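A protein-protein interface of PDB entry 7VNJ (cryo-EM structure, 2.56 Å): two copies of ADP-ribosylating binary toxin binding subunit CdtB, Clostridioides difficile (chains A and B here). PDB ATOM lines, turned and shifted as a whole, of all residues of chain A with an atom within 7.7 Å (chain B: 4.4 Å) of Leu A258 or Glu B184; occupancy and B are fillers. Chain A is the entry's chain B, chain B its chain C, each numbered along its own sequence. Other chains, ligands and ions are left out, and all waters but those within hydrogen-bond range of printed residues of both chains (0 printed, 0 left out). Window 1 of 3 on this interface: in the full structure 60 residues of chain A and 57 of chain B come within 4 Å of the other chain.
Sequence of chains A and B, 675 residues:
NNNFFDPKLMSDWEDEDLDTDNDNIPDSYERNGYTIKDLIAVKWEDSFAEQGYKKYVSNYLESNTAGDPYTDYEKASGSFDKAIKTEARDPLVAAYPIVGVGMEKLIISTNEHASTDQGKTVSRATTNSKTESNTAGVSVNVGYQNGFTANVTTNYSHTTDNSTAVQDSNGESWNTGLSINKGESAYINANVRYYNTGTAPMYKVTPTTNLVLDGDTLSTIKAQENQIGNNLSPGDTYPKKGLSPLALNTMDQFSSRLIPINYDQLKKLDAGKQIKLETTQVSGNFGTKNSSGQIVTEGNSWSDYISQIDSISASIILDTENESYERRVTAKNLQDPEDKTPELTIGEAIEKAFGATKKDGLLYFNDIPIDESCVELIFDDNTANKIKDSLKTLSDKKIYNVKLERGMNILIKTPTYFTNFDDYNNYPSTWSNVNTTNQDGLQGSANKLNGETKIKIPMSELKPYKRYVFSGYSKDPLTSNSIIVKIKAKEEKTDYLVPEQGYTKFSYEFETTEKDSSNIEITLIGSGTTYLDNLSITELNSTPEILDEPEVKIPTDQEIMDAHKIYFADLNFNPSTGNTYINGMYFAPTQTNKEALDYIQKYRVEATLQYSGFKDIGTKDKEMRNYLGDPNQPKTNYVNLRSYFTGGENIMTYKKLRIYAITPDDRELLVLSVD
OD1 of Asn B181 lies close to O of Glu A112 (3.3 Å). O of Glu A112 sits at hydrogen-bond distance from N of Lys B182 (2.8 Å). The backbone NH (N) of Gly B183 is in hydrogen-bond range of the backbone carbonyl oxygen (O) of Thr A110, at 3.2 Å. The side-chain amide oxygen (OD1) of Asn A111 sits close to the side-chain amide oxygen (OD1) of Asn B181, 3.3 Å away. A ring nitrogen (NE2) of His A113 sits close to the side-chain amide nitrogen (ND2) of Asn B181, at 3.3 Å.
Along chain B the printed residues that touch a printed residue of chain A span positions 181 to 257. Among the printed residues, 8 pairs touch across the chains. Among the printed residues, no Asp or Glu carboxylate lies within 4 Å of a Lys or Arg side-chain nitrogen of the other chain.
O of Glu B184 lies within hydrogen-bond range of ND2 of Asn B111. OE2 of Glu B184 lies within salt-bridge range of NH2 of Arg B257, at 2.8 Å. The side-chain carboxylate of Asp A252 lies within hydrogen-bond range of the backbone NH of Ser A256, at 2.5 Å. N of Gly B183 lies within hydrogen-bond range of OD1 of Asn B181. The backbone carbonyl oxygen (O) of Asn B181 lies within hydrogen-bond range of the side-chain hydroxyl (OG) of Ser B185, 2.8 Å away. ND2 of Asn A111 sits at hydrogen-bond distance from O of Glu A184 (3.3 Å).
Thr A110 touches Lys B182. Ser A256 touches Arg B257 (O to NE, 3.7 Å). Glu B184 touches Leu A258 (OE2 to CD1, 3.8 Å).
Positions printed for both chains: 111, 184, 186, 187, 257, 260 and 261. Of the 8 pairs that touch across the chains among the printed residues, none has its exchanged pair printed and touching as well.
Of the printed residues of chain B, Asn A111 touches Asn B181 (3.3 Å). Of the printed residues of chain B, Ser A256 touches Arg B257 (3.7 Å). Leu A258 touches just one residue of chain B: Glu B184 (3.8 Å). Pro A260 touches none of the printed residues of chain B. Of the printed residues of chain A, Asn B181 touches Asn A111, Glu A112 and His A113. Of chain A, only Leu A258 (3.8 Å) comes within 4 Å of Glu B184. Ser B185 touches none of the printed residues of chain A. The nearest residue of chain B that does not touch Leu A258 is Arg B257 (4.1 Å). The nearest printed residue of chain B that does not touch Ser A256 is Glu B184 (7.4 Å).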
ATOM      1  N   SER A 109      -4.787 -15.365 -15.154  1.00  0.00           N
ATOM      2  CA  SER A 109      -4.581 -16.782 -14.862  1.00  0.00           C
ATOM      3  C   SER A 109      -5.306 -17.114 -13.563  1.00  0.00           C
ATOM      4  O   SER A 109      -4.778 -16.867 -12.475  1.00  0.00           O
ATOM      5  CB  SER A 109      -3.095 -17.098 -14.750  1.00  0.00           C
ATOM      6  OG  SER A 109      -2.452 -16.993 -16.006  1.00  0.00           O
ATOM      7  N   THR A 110      -6.504 -17.683 -13.669  1.00  0.00           N
ATOM      8  CA  THR A 110      -7.267 -18.035 -12.479  1.00  0.00           C
ATOM      9  C   THR A 110      -6.569 -19.154 -11.719  1.00  0.00           C
ATOM     10  O   THR A 110      -6.155 -20.156 -12.308  1.00  0.00           O
ATOM     11  CB  THR A 110      -8.684 -18.459 -12.857  1.00  0.00           C
ATOM     12  OG1 THR A 110      -9.207 -17.558 -13.840  1.00  0.00           O
ATOM     13  CG2 THR A 110      -9.582 -18.434 -11.636  1.00  0.00           C
ATOM     14  N   ASN A 111      -6.442 -18.984 -10.406  1.00  0.00           N
ATOM     15  CA  ASN A 111      -5.713 -19.920  -9.553  1.00  0.00           C
ATOM     16  C   ASN A 111      -6.731 -20.793  -8.827  1.00  0.00           C
ATOM     17  O   ASN A 111      -7.123 -20.515  -7.695  1.00  0.00           O
ATOM     18  CB  ASN A 111      -4.814 -19.167  -8.581  1.00  0.00           C
ATOM     19  CG  ASN A 111      -3.918 -20.087  -7.782  1.00  0.00           C
ATOM     20  OD1 ASN A 111      -3.487 -21.129  -8.272  1.00  0.00           O
ATOM     21  ND2 ASN A 111      -3.629 -19.704  -6.545  1.00  0.00           N
ATOM     22  N   GLU A 112      -7.156 -21.867  -9.489  1.00  0.00           N
ATOM     23  CA  GLU A 112      -8.156 -22.775  -8.951  1.00  0.00           C
ATOM     24  C   GLU A 112      -7.637 -24.203  -8.988  1.00  0.00           C
ATOM     25  O   GLU A 112      -6.843 -24.571  -9.856  1.00  0.00           O
ATOM     26  CB  GLU A 112      -9.471 -22.695  -9.731  1.00  0.00           C
ATOM     27  CG  GLU A 112     -10.308 -21.475  -9.419  1.00  0.00           C
ATOM     28  CD  GLU A 112     -11.531 -21.377 -10.304  1.00  0.00           C
ATOM     29  OE1 GLU A 112     -11.522 -21.975 -11.400  1.00  0.00           O
ATOM     30  OE2 GLU A 112     -12.503 -20.704  -9.904  1.00  0.00           O
ATOM     31  N   HIS A 113      -8.087 -24.999  -8.023  1.00  0.00           N
ATOM     32  CA  HIS A 113      -7.758 -26.414  -7.937  1.00  0.00           C
ATOM     33  C   HIS A 113      -9.009 -27.230  -8.217  1.00  0.00           C
ATOM     34  O   HIS A 113     -10.044 -27.024  -7.578  1.00  0.00           O
ATOM     35  CB  HIS A 113      -7.203 -26.768  -6.557  1.00  0.00           C
ATOM     36  CG  HIS A 113      -5.798 -26.309  -6.335  1.00  0.00           C
ATOM     37  ND1 HIS A 113      -4.703 -27.086  -6.649  1.00  0.00           N
ATOM     38  CD2 HIS A 113      -5.307 -25.153  -5.830  1.00  0.00           C
ATOM     39  CE1 HIS A 113      -3.599 -26.428  -6.346  1.00  0.00           C
ATOM     40  NE2 HIS A 113      -3.937 -25.253  -5.849  1.00  0.00           N
ATOM     41  N   GLU A 184      -5.072 -14.973  -2.972  1.00  0.00           N
ATOM     42  CA  GLU A 184      -4.454 -14.952  -4.298  1.00  0.00           C
ATOM     43  C   GLU A 184      -5.361 -15.741  -5.235  1.00  0.00           C
ATOM     44  O   GLU A 184      -5.151 -16.935  -5.454  1.00  0.00           O
ATOM     45  CB  GLU A 184      -3.045 -15.531  -4.259  1.00  0.00           C
ATOM     46  CG  GLU A 184      -2.178 -14.990  -3.138  1.00  0.00           C
ATOM     47  CD  GLU A 184      -0.698 -15.094  -3.444  1.00  0.00           C
ATOM     48  OE1 GLU A 184      -0.345 -15.714  -4.468  1.00  0.00           O
ATOM     49  OE2 GLU A 184       0.112 -14.557  -2.661  1.00  0.00           O
ATOM     50  N   ALA A 186      -5.996 -15.045  -8.573  1.00  0.00           N
ATOM     51  CA  ALA A 186      -5.549 -15.136  -9.955  1.00  0.00           C
ATOM     52  C   ALA A 186      -4.223 -14.407 -10.106  1.00  0.00           C
ATOM     53  O   ALA A 186      -3.807 -13.643  -9.232  1.00  0.00           O
ATOM     54  CB  ALA A 186      -6.596 -14.570 -10.918  1.00  0.00           C
ATOM     55  N   TYR A 187      -3.563 -14.661 -11.232  1.00  0.00           N
ATOM     56  CA  TYR A 187      -2.332 -13.986 -11.607  1.00  0.00           C
ATOM     57  C   TYR A 187      -2.546 -13.237 -12.914  1.00  0.00           C
ATOM     58  O   TYR A 187      -3.330 -13.660 -13.767  1.00  0.00           O
ATOM     59  CB  TYR A 187      -1.176 -14.976 -11.758  1.00  0.00           C
ATOM     60  CG  TYR A 187      -0.825 -15.696 -10.482  1.00  0.00           C
ATOM     61  CD1 TYR A 187      -0.456 -14.992  -9.347  1.00  0.00           C
ATOM     62  CD2 TYR A 187      -0.862 -17.081 -10.412  1.00  0.00           C
ATOM     63  CE1 TYR A 187      -0.133 -15.643  -8.178  1.00  0.00           C
ATOM     64  CE2 TYR A 187      -0.540 -17.741  -9.244  1.00  0.00           C
ATOM     65  CZ  TYR A 187      -0.177 -17.017  -8.131  1.00  0.00           C
ATOM     66  OH  TYR A 187       0.145 -17.668  -6.965  1.00  0.00           O
ATOM     67  N   ILE A 188      -1.843 -12.119 -13.067  1.00  0.00           N
ATOM     68  CA  ILE A 188      -2.018 -11.231 -14.209  1.00  0.00           C
ATOM     69  C   ILE A 188      -0.710 -11.138 -14.979  1.00  0.00           C
ATOM     70  O   ILE A 188       0.374 -11.113 -14.388  1.00  0.00           O
ATOM     71  CB  ILE A 188      -2.495  -9.831 -13.774  1.00  0.00           C
ATOM     72  CG1 ILE A 188      -1.663  -9.324 -12.597  1.00  0.00           C
ATOM     73  CG2 ILE A 188      -3.967  -9.862 -13.416  1.00  0.00           C
ATOM     74  CD1 ILE A 188      -2.035  -7.935 -12.151  1.00  0.00           C
ATOM     75  N   ASN A 249       5.255 -10.297 -15.926  1.00  0.00           N
ATOM     76  CA  ASN A 249       4.446 -11.229 -15.152  1.00  0.00           C
ATOM     77  C   ASN A 249       5.077 -11.622 -13.822  1.00  0.00           C
ATOM     78  O   ASN A 249       4.612 -12.579 -13.194  1.00  0.00           O
ATOM     79  CB  ASN A 249       4.153 -12.487 -15.975  1.00  0.00           C
ATOM     80  CG  ASN A 249       5.413 -13.181 -16.442  1.00  0.00           C
ATOM     81  OD1 ASN A 249       6.515 -12.656 -16.296  1.00  0.00           O
ATOM     82  ND2 ASN A 249       5.258 -14.368 -17.010  1.00  0.00           N
ATOM     83  N   THR A 250       6.114 -10.922 -13.375  1.00  0.00           N
ATOM     84  CA  THR A 250       6.745 -11.203 -12.096  1.00  0.00           C
ATOM     85  C   THR A 250       6.954  -9.904 -11.336  1.00  0.00           C
ATOM     86  O   THR A 250       7.096  -8.834 -11.933  1.00  0.00           O
ATOM     87  CB  THR A 250       8.088 -11.928 -12.264  1.00  0.00           C
ATOM     88  OG1 THR A 250       8.926 -11.189 -13.160  1.00  0.00           O
ATOM     89  CG2 THR A 250       7.877 -13.331 -12.808  1.00  0.00           C
ATOM     90  N   MET A 251       6.973 -10.008 -10.008  1.00  0.00           N
ATOM     91  CA  MET A 251       7.077  -8.843  -9.144  1.00  0.00           C
ATOM     92  C   MET A 251       8.303  -8.832  -8.246  1.00  0.00           C
ATOM     93  O   MET A 251       8.704  -7.752  -7.803  1.00  0.00           O
ATOM     94  CB  MET A 251       5.826  -8.717  -8.260  1.00  0.00           C
ATOM     95  CG  MET A 251       5.655  -9.854  -7.271  1.00  0.00           C
ATOM     96  SD  MET A 251       4.192  -9.676  -6.235  1.00  0.00           S
ATOM     97  CE  MET A 251       4.702  -8.337  -5.165  1.00  0.00           C
ATOM     98  N   ASP A 252       8.907  -9.981  -7.962  1.00  0.00           N
ATOM     99  CA  ASP A 252      10.042 -10.000  -7.056  1.00  0.00           C
ATOM    100  C   ASP A 252      11.330  -9.665  -7.804  1.00  0.00           C
ATOM    101  O   ASP A 252      11.356  -9.523  -9.028  1.00  0.00           O
ATOM    102  CB  ASP A 252      10.154 -11.355  -6.361  1.00  0.00           C
ATOM    103  CG  ASP A 252      10.721 -12.427  -7.261  1.00  0.00           C
ATOM    104  OD1 ASP A 252      10.285 -12.513  -8.426  1.00  0.00           O
ATOM    105  OD2 ASP A 252      11.599 -13.185  -6.802  1.00  0.00           O
ATOM    106  N   SER A 255      12.546 -12.507 -10.369  1.00  0.00           N
ATOM    107  CA  SER A 255      11.582 -13.008 -11.352  1.00  0.00           C
ATOM    108  C   SER A 255      11.091 -14.410 -10.997  1.00  0.00           C
ATOM    109  O   SER A 255      10.948 -15.273 -11.864  1.00  0.00           O
ATOM    110  CB  SER A 255      12.170 -12.983 -12.764  1.00  0.00           C
ATOM    111  OG  SER A 255      12.792 -11.743 -13.038  1.00  0.00           O
ATOM    112  N   SER A 256      10.825 -14.638  -9.714  1.00  0.00           N
ATOM    113  CA  SER A 256      10.397 -15.944  -9.236  1.00  0.00           C
ATOM    114  C   SER A 256       9.016 -15.942  -8.597  1.00  0.00           C
ATOM    115  O   SER A 256       8.581 -16.988  -8.105  1.00  0.00           O
ATOM    116  CB  SER A 256      11.415 -16.496  -8.231  1.00  0.00           C
ATOM    117  OG  SER A 256      10.960 -17.712  -7.670  1.00  0.00           O
ATOM    118  N   ARG A 257       8.313 -14.811  -8.589  1.00  0.00           N
ATOM    119  CA  ARG A 257       7.001 -14.707  -7.964  1.00  0.00           C
ATOM    120  C   ARG A 257       6.057 -13.966  -8.896  1.00  0.00           C
ATOM    121  O   ARG A 257       6.393 -12.887  -9.390  1.00  0.00           O
ATOM    122  CB  ARG A 257       7.093 -13.983  -6.618  1.00  0.00           C
ATOM    123  CG  ARG A 257       6.062 -14.422  -5.602  1.00  0.00           C
ATOM    124  CD  ARG A 257       5.593 -13.249  -4.768  1.00  0.00           C
ATOM    125  NE  ARG A 257       4.803 -13.677  -3.620  1.00  0.00           N
ATOM    126  CZ  ARG A 257       3.524 -14.020  -3.679  1.00  0.00           C
ATOM    127  NH1 ARG A 257       2.855 -13.999  -4.819  1.00  0.00           N
ATOM    128  NH2 ARG A 257       2.901 -14.393  -2.566  1.00  0.00           N
ATOM    129  N   LEU A 258       4.879 -14.539  -9.128  1.00  0.00           N
ATOM    130  CA  LEU A 258       3.902 -13.943 -10.023  1.00  0.00           C
ATOM    131  C   LEU A 258       3.159 -12.806  -9.321  1.00  0.00           C
ATOM    132  O   LEU A 258       3.341 -12.550  -8.129  1.00  0.00           O
ATOM    133  CB  LEU A 258       2.937 -15.008 -10.535  1.00  0.00           C
ATOM    134  CG  LEU A 258       3.582 -16.251 -11.149  1.00  0.00           C
ATOM    135  CD1 LEU A 258       2.528 -17.261 -11.551  1.00  0.00           C
ATOM    136  CD2 LEU A 258       4.445 -15.880 -12.341  1.00  0.00           C
ATOM    137  N   ILE A 259       2.304 -12.115 -10.071  1.00  0.00           N
ATOM    138  CA  ILE A 259       1.591 -10.939  -9.580  1.00  0.00           C
ATOM    139  C   ILE A 259       0.167 -11.366  -9.233  1.00  0.00           C
ATOM    140  O   ILE A 259      -0.615 -11.669 -10.148  1.00  0.00           O
ATOM    141  CB  ILE A 259       1.595  -9.809 -10.616  1.00  0.00           C
ATOM    142  CG1 ILE A 259       3.002  -9.606 -11.175  1.00  0.00           C
ATOM    143  CG2 ILE A 259       1.078  -8.522 -10.004  1.00  0.00           C
ATOM    144  CD1 ILE A 259       3.050  -8.712 -12.385  1.00  0.00           C
ATOM    145  N   PRO A 260      -0.212 -11.397  -7.959  1.00  0.00           N
ATOM    146  CA  PRO A 260      -1.547 -11.866  -7.580  1.00  0.00           C
ATOM    147  C   PRO A 260      -2.566 -10.742  -7.451  1.00  0.00           C
ATOM    148  O   PRO A 260      -2.231  -9.562  -7.350  1.00  0.00           O
ATOM    149  CB  PRO A 260      -1.291 -12.519  -6.218  1.00  0.00           C
ATOM    150  CG  PRO A 260      -0.181 -11.698  -5.635  1.00  0.00           C
ATOM    151  CD  PRO A 260       0.624 -11.122  -6.780  1.00  0.00           C
ATOM    152  N   ILE A 261      -3.840 -11.145  -7.454  1.00  0.00           N
ATOM    153  CA  ILE A 261      -4.962 -10.250  -7.200  1.00  0.00           C
ATOM    154  C   ILE A 261      -5.938 -10.946  -6.259  1.00  0.00           C
ATOM    155  O   ILE A 261      -5.890 -12.162  -6.067  1.00  0.00           O
ATOM    156  CB  ILE A 261      -5.687  -9.816  -8.493  1.00  0.00           C
ATOM    157  CG1 ILE A 261      -6.116 -11.038  -9.301  1.00  0.00           C
ATOM    158  CG2 ILE A 261      -4.803  -8.912  -9.325  1.00  0.00           C
ATOM    159  CD1 ILE A 261      -7.004 -10.702 -10.469  1.00  0.00           C
ATOM    160  N   ASN B 111       1.099 -30.899 -15.542  1.00  0.00           N
ATOM    161  CA  ASN B 111       1.254 -30.889 -14.089  1.00  0.00           C
ATOM    162  C   ASN B 111      -0.022 -31.437 -13.456  1.00  0.00           C
ATOM    163  O   ASN B 111      -0.907 -30.699 -13.027  1.00  0.00           O
ATOM    164  CB  ASN B 111       1.572 -29.479 -13.605  1.00  0.00           C
ATOM    165  CG  ASN B 111       2.004 -29.442 -12.156  1.00  0.00           C
ATOM    166  OD1 ASN B 111       2.622 -30.379 -11.656  1.00  0.00           O
ATOM    167  ND2 ASN B 111       1.681 -28.351 -11.472  1.00  0.00           N
ATOM    168  N   ASN B 181      -4.223 -28.006 -11.284  1.00  0.00           N
ATOM    169  CA  ASN B 181      -4.199 -26.589 -10.946  1.00  0.00           C
ATOM    170  C   ASN B 181      -4.428 -25.787 -12.220  1.00  0.00           C
ATOM    171  O   ASN B 181      -3.685 -25.938 -13.194  1.00  0.00           O
ATOM    172  CB  ASN B 181      -2.869 -26.207 -10.297  1.00  0.00           C
ATOM    173  CG  ASN B 181      -2.918 -24.859  -9.610  1.00  0.00           C
ATOM    174  OD1 ASN B 181      -3.651 -23.962 -10.021  1.00  0.00           O
ATOM    175  ND2 ASN B 181      -2.129 -24.708  -8.556  1.00  0.00           N
ATOM    176  N   LYS B 182      -5.453 -24.937 -12.211  1.00  0.00           N
ATOM    177  CA  LYS B 182      -5.783 -24.157 -13.396  1.00  0.00           C
ATOM    178  C   LYS B 182      -4.835 -22.988 -13.616  1.00  0.00           C
ATOM    179  O   LYS B 182      -4.797 -22.442 -14.724  1.00  0.00           O
ATOM    180  CB  LYS B 182      -7.220 -23.645 -13.303  1.00  0.00           C
ATOM    181  CG  LYS B 182      -8.249 -24.739 -13.099  1.00  0.00           C
ATOM    182  CD  LYS B 182      -8.300 -25.676 -14.290  1.00  0.00           C
ATOM    183  CE  LYS B 182      -9.677 -26.295 -14.441  1.00  0.00           C
ATOM    184  NZ  LYS B 182     -10.751 -25.270 -14.369  1.00  0.00           N
ATOM    185  N   GLY B 183      -4.074 -22.592 -12.601  1.00  0.00           N
ATOM    186  CA  GLY B 183      -3.130 -21.504 -12.751  1.00  0.00           C
ATOM    187  C   GLY B 183      -1.843 -21.940 -13.417  1.00  0.00           C
ATOM    188  O   GLY B 183      -1.337 -21.259 -14.315  1.00  0.00           O
ATOM    189  N   GLU B 184      -1.302 -23.078 -12.987  1.00  0.00           N
ATOM    190  CA  GLU B 184      -0.085 -23.658 -13.555  1.00  0.00           C
ATOM    191  C   GLU B 184      -0.415 -25.095 -13.940  1.00  0.00           C
ATOM    192  O   GLU B 184      -0.193 -26.022 -13.157  1.00  0.00           O
ATOM    193  CB  GLU B 184       1.071 -23.591 -12.566  1.00  0.00           C
ATOM    194  CG  GLU B 184       1.282 -22.223 -11.948  1.00  0.00           C
ATOM    195  CD  GLU B 184       2.637 -22.087 -11.287  1.00  0.00           C
ATOM    196  OE1 GLU B 184       3.298 -23.125 -11.067  1.00  0.00           O
ATOM    197  OE2 GLU B 184       3.044 -20.945 -10.989  1.00  0.00           O
ATOM    198  N   SER B 185      -0.940 -25.279 -15.148  1.00  0.00           N
ATOM    199  CA  SER B 185      -1.386 -26.593 -15.584  1.00  0.00           C
ATOM    200  C   SER B 185      -0.301 -27.402 -16.274  1.00  0.00           C
ATOM    201  O   SER B 185      -0.405 -28.632 -16.322  1.00  0.00           O
ATOM    202  CB  SER B 185      -2.586 -26.454 -16.523  1.00  0.00           C
ATOM    203  OG  SER B 185      -3.551 -25.573 -15.978  1.00  0.00           O
ATOM    204  N   ALA B 186       0.731 -26.755 -16.809  1.00  0.00           N
ATOM    205  CA  ALA B 186       1.783 -27.474 -17.509  1.00  0.00           C
ATOM    206  C   ALA B 186       3.046 -26.629 -17.522  1.00  0.00           C
ATOM    207  O   ALA B 186       3.013 -25.425 -17.258  1.00  0.00           O
ATOM    208  CB  ALA B 186       1.363 -27.836 -18.936  1.00  0.00           C
ATOM    209  N   TYR B 187       4.161 -27.282 -17.832  1.00  0.00           N
ATOM    210  CA  TYR B 187       5.448 -26.627 -18.000  1.00  0.00           C
ATOM    211  C   TYR B 187       5.946 -26.852 -19.420  1.00  0.00           C
ATOM    212  O   TYR B 187       5.689 -27.895 -20.025  1.00  0.00           O
ATOM    213  CB  TYR B 187       6.482 -27.151 -17.002  1.00  0.00           C
ATOM    214  CG  TYR B 187       6.142 -26.878 -15.559  1.00  0.00           C
ATOM    215  CD1 TYR B 187       5.931 -25.585 -15.111  1.00  0.00           C
ATOM    216  CD2 TYR B 187       6.042 -27.913 -14.642  1.00  0.00           C
ATOM    217  CE1 TYR B 187       5.623 -25.329 -13.793  1.00  0.00           C
ATOM    218  CE2 TYR B 187       5.735 -27.668 -13.322  1.00  0.00           C
ATOM    219  CZ  TYR B 187       5.527 -26.374 -12.901  1.00  0.00           C
ATOM    220  OH  TYR B 187       5.221 -26.123 -11.586  1.00  0.00           O
ATOM    221  N   ARG B 257      13.159 -22.126 -11.199  1.00  0.00           N
ATOM    222  CA  ARG B 257      11.726 -21.981 -11.421  1.00  0.00           C
ATOM    223  C   ARG B 257      11.408 -22.353 -12.860  1.00  0.00           C
ATOM    224  O   ARG B 257      12.045 -21.845 -13.785  1.00  0.00           O
ATOM    225  CB  ARG B 257      11.279 -20.546 -11.132  1.00  0.00           C
ATOM    226  CG  ARG B 257       9.786 -20.305 -11.214  1.00  0.00           C
ATOM    227  CD  ARG B 257       9.076 -20.721  -9.942  1.00  0.00           C
ATOM    228  NE  ARG B 257       7.743 -20.135  -9.847  1.00  0.00           N
ATOM    229  CZ  ARG B 257       6.710 -20.486 -10.600  1.00  0.00           C
ATOM    230  NH1 ARG B 257       6.810 -21.432 -11.518  1.00  0.00           N
ATOM    231  NH2 ARG B 257       5.543 -19.872 -10.423  1.00  0.00           N
ATOM    232  N   PRO B 260       5.603 -21.870 -16.523  1.00  0.00           N
ATOM    233  CA  PRO B 260       4.233 -22.382 -16.494  1.00  0.00           C
ATOM    234  C   PRO B 260       3.360 -21.804 -17.604  1.00  0.00           C
ATOM    235  O   PRO B 260       3.694 -20.804 -18.240  1.00  0.00           O
ATOM    236  CB  PRO B 260       3.737 -21.920 -15.123  1.00  0.00           C
ATOM    237  CG  PRO B 260       4.458 -20.625 -14.901  1.00  0.00           C
ATOM    238  CD  PRO B 260       5.758 -20.679 -15.672  1.00  0.00           C
ATOM    239  N   ILE B 261       2.218 -22.461 -17.818  1.00  0.00           N
ATOM    240  CA  ILE B 261       1.170 -21.982 -18.713  1.00  0.00           C
ATOM    241  C   ILE B 261      -0.181 -22.215 -18.046  1.00  0.00           C
ATOM    242  O   ILE B 261      -0.292 -22.915 -17.039  1.00  0.00           O
ATOM    243  CB  ILE B 261       1.205 -22.667 -20.095  1.00  0.00           C
ATOM    244  CG1 ILE B 261       1.135 -24.184 -19.944  1.00  0.00           C
ATOM    245  CG2 ILE B 261       2.443 -22.258 -20.867  1.00  0.00           C
ATOM    246  CD1 ILE B 261       0.869 -24.902 -21.239  1.00  0.00           C
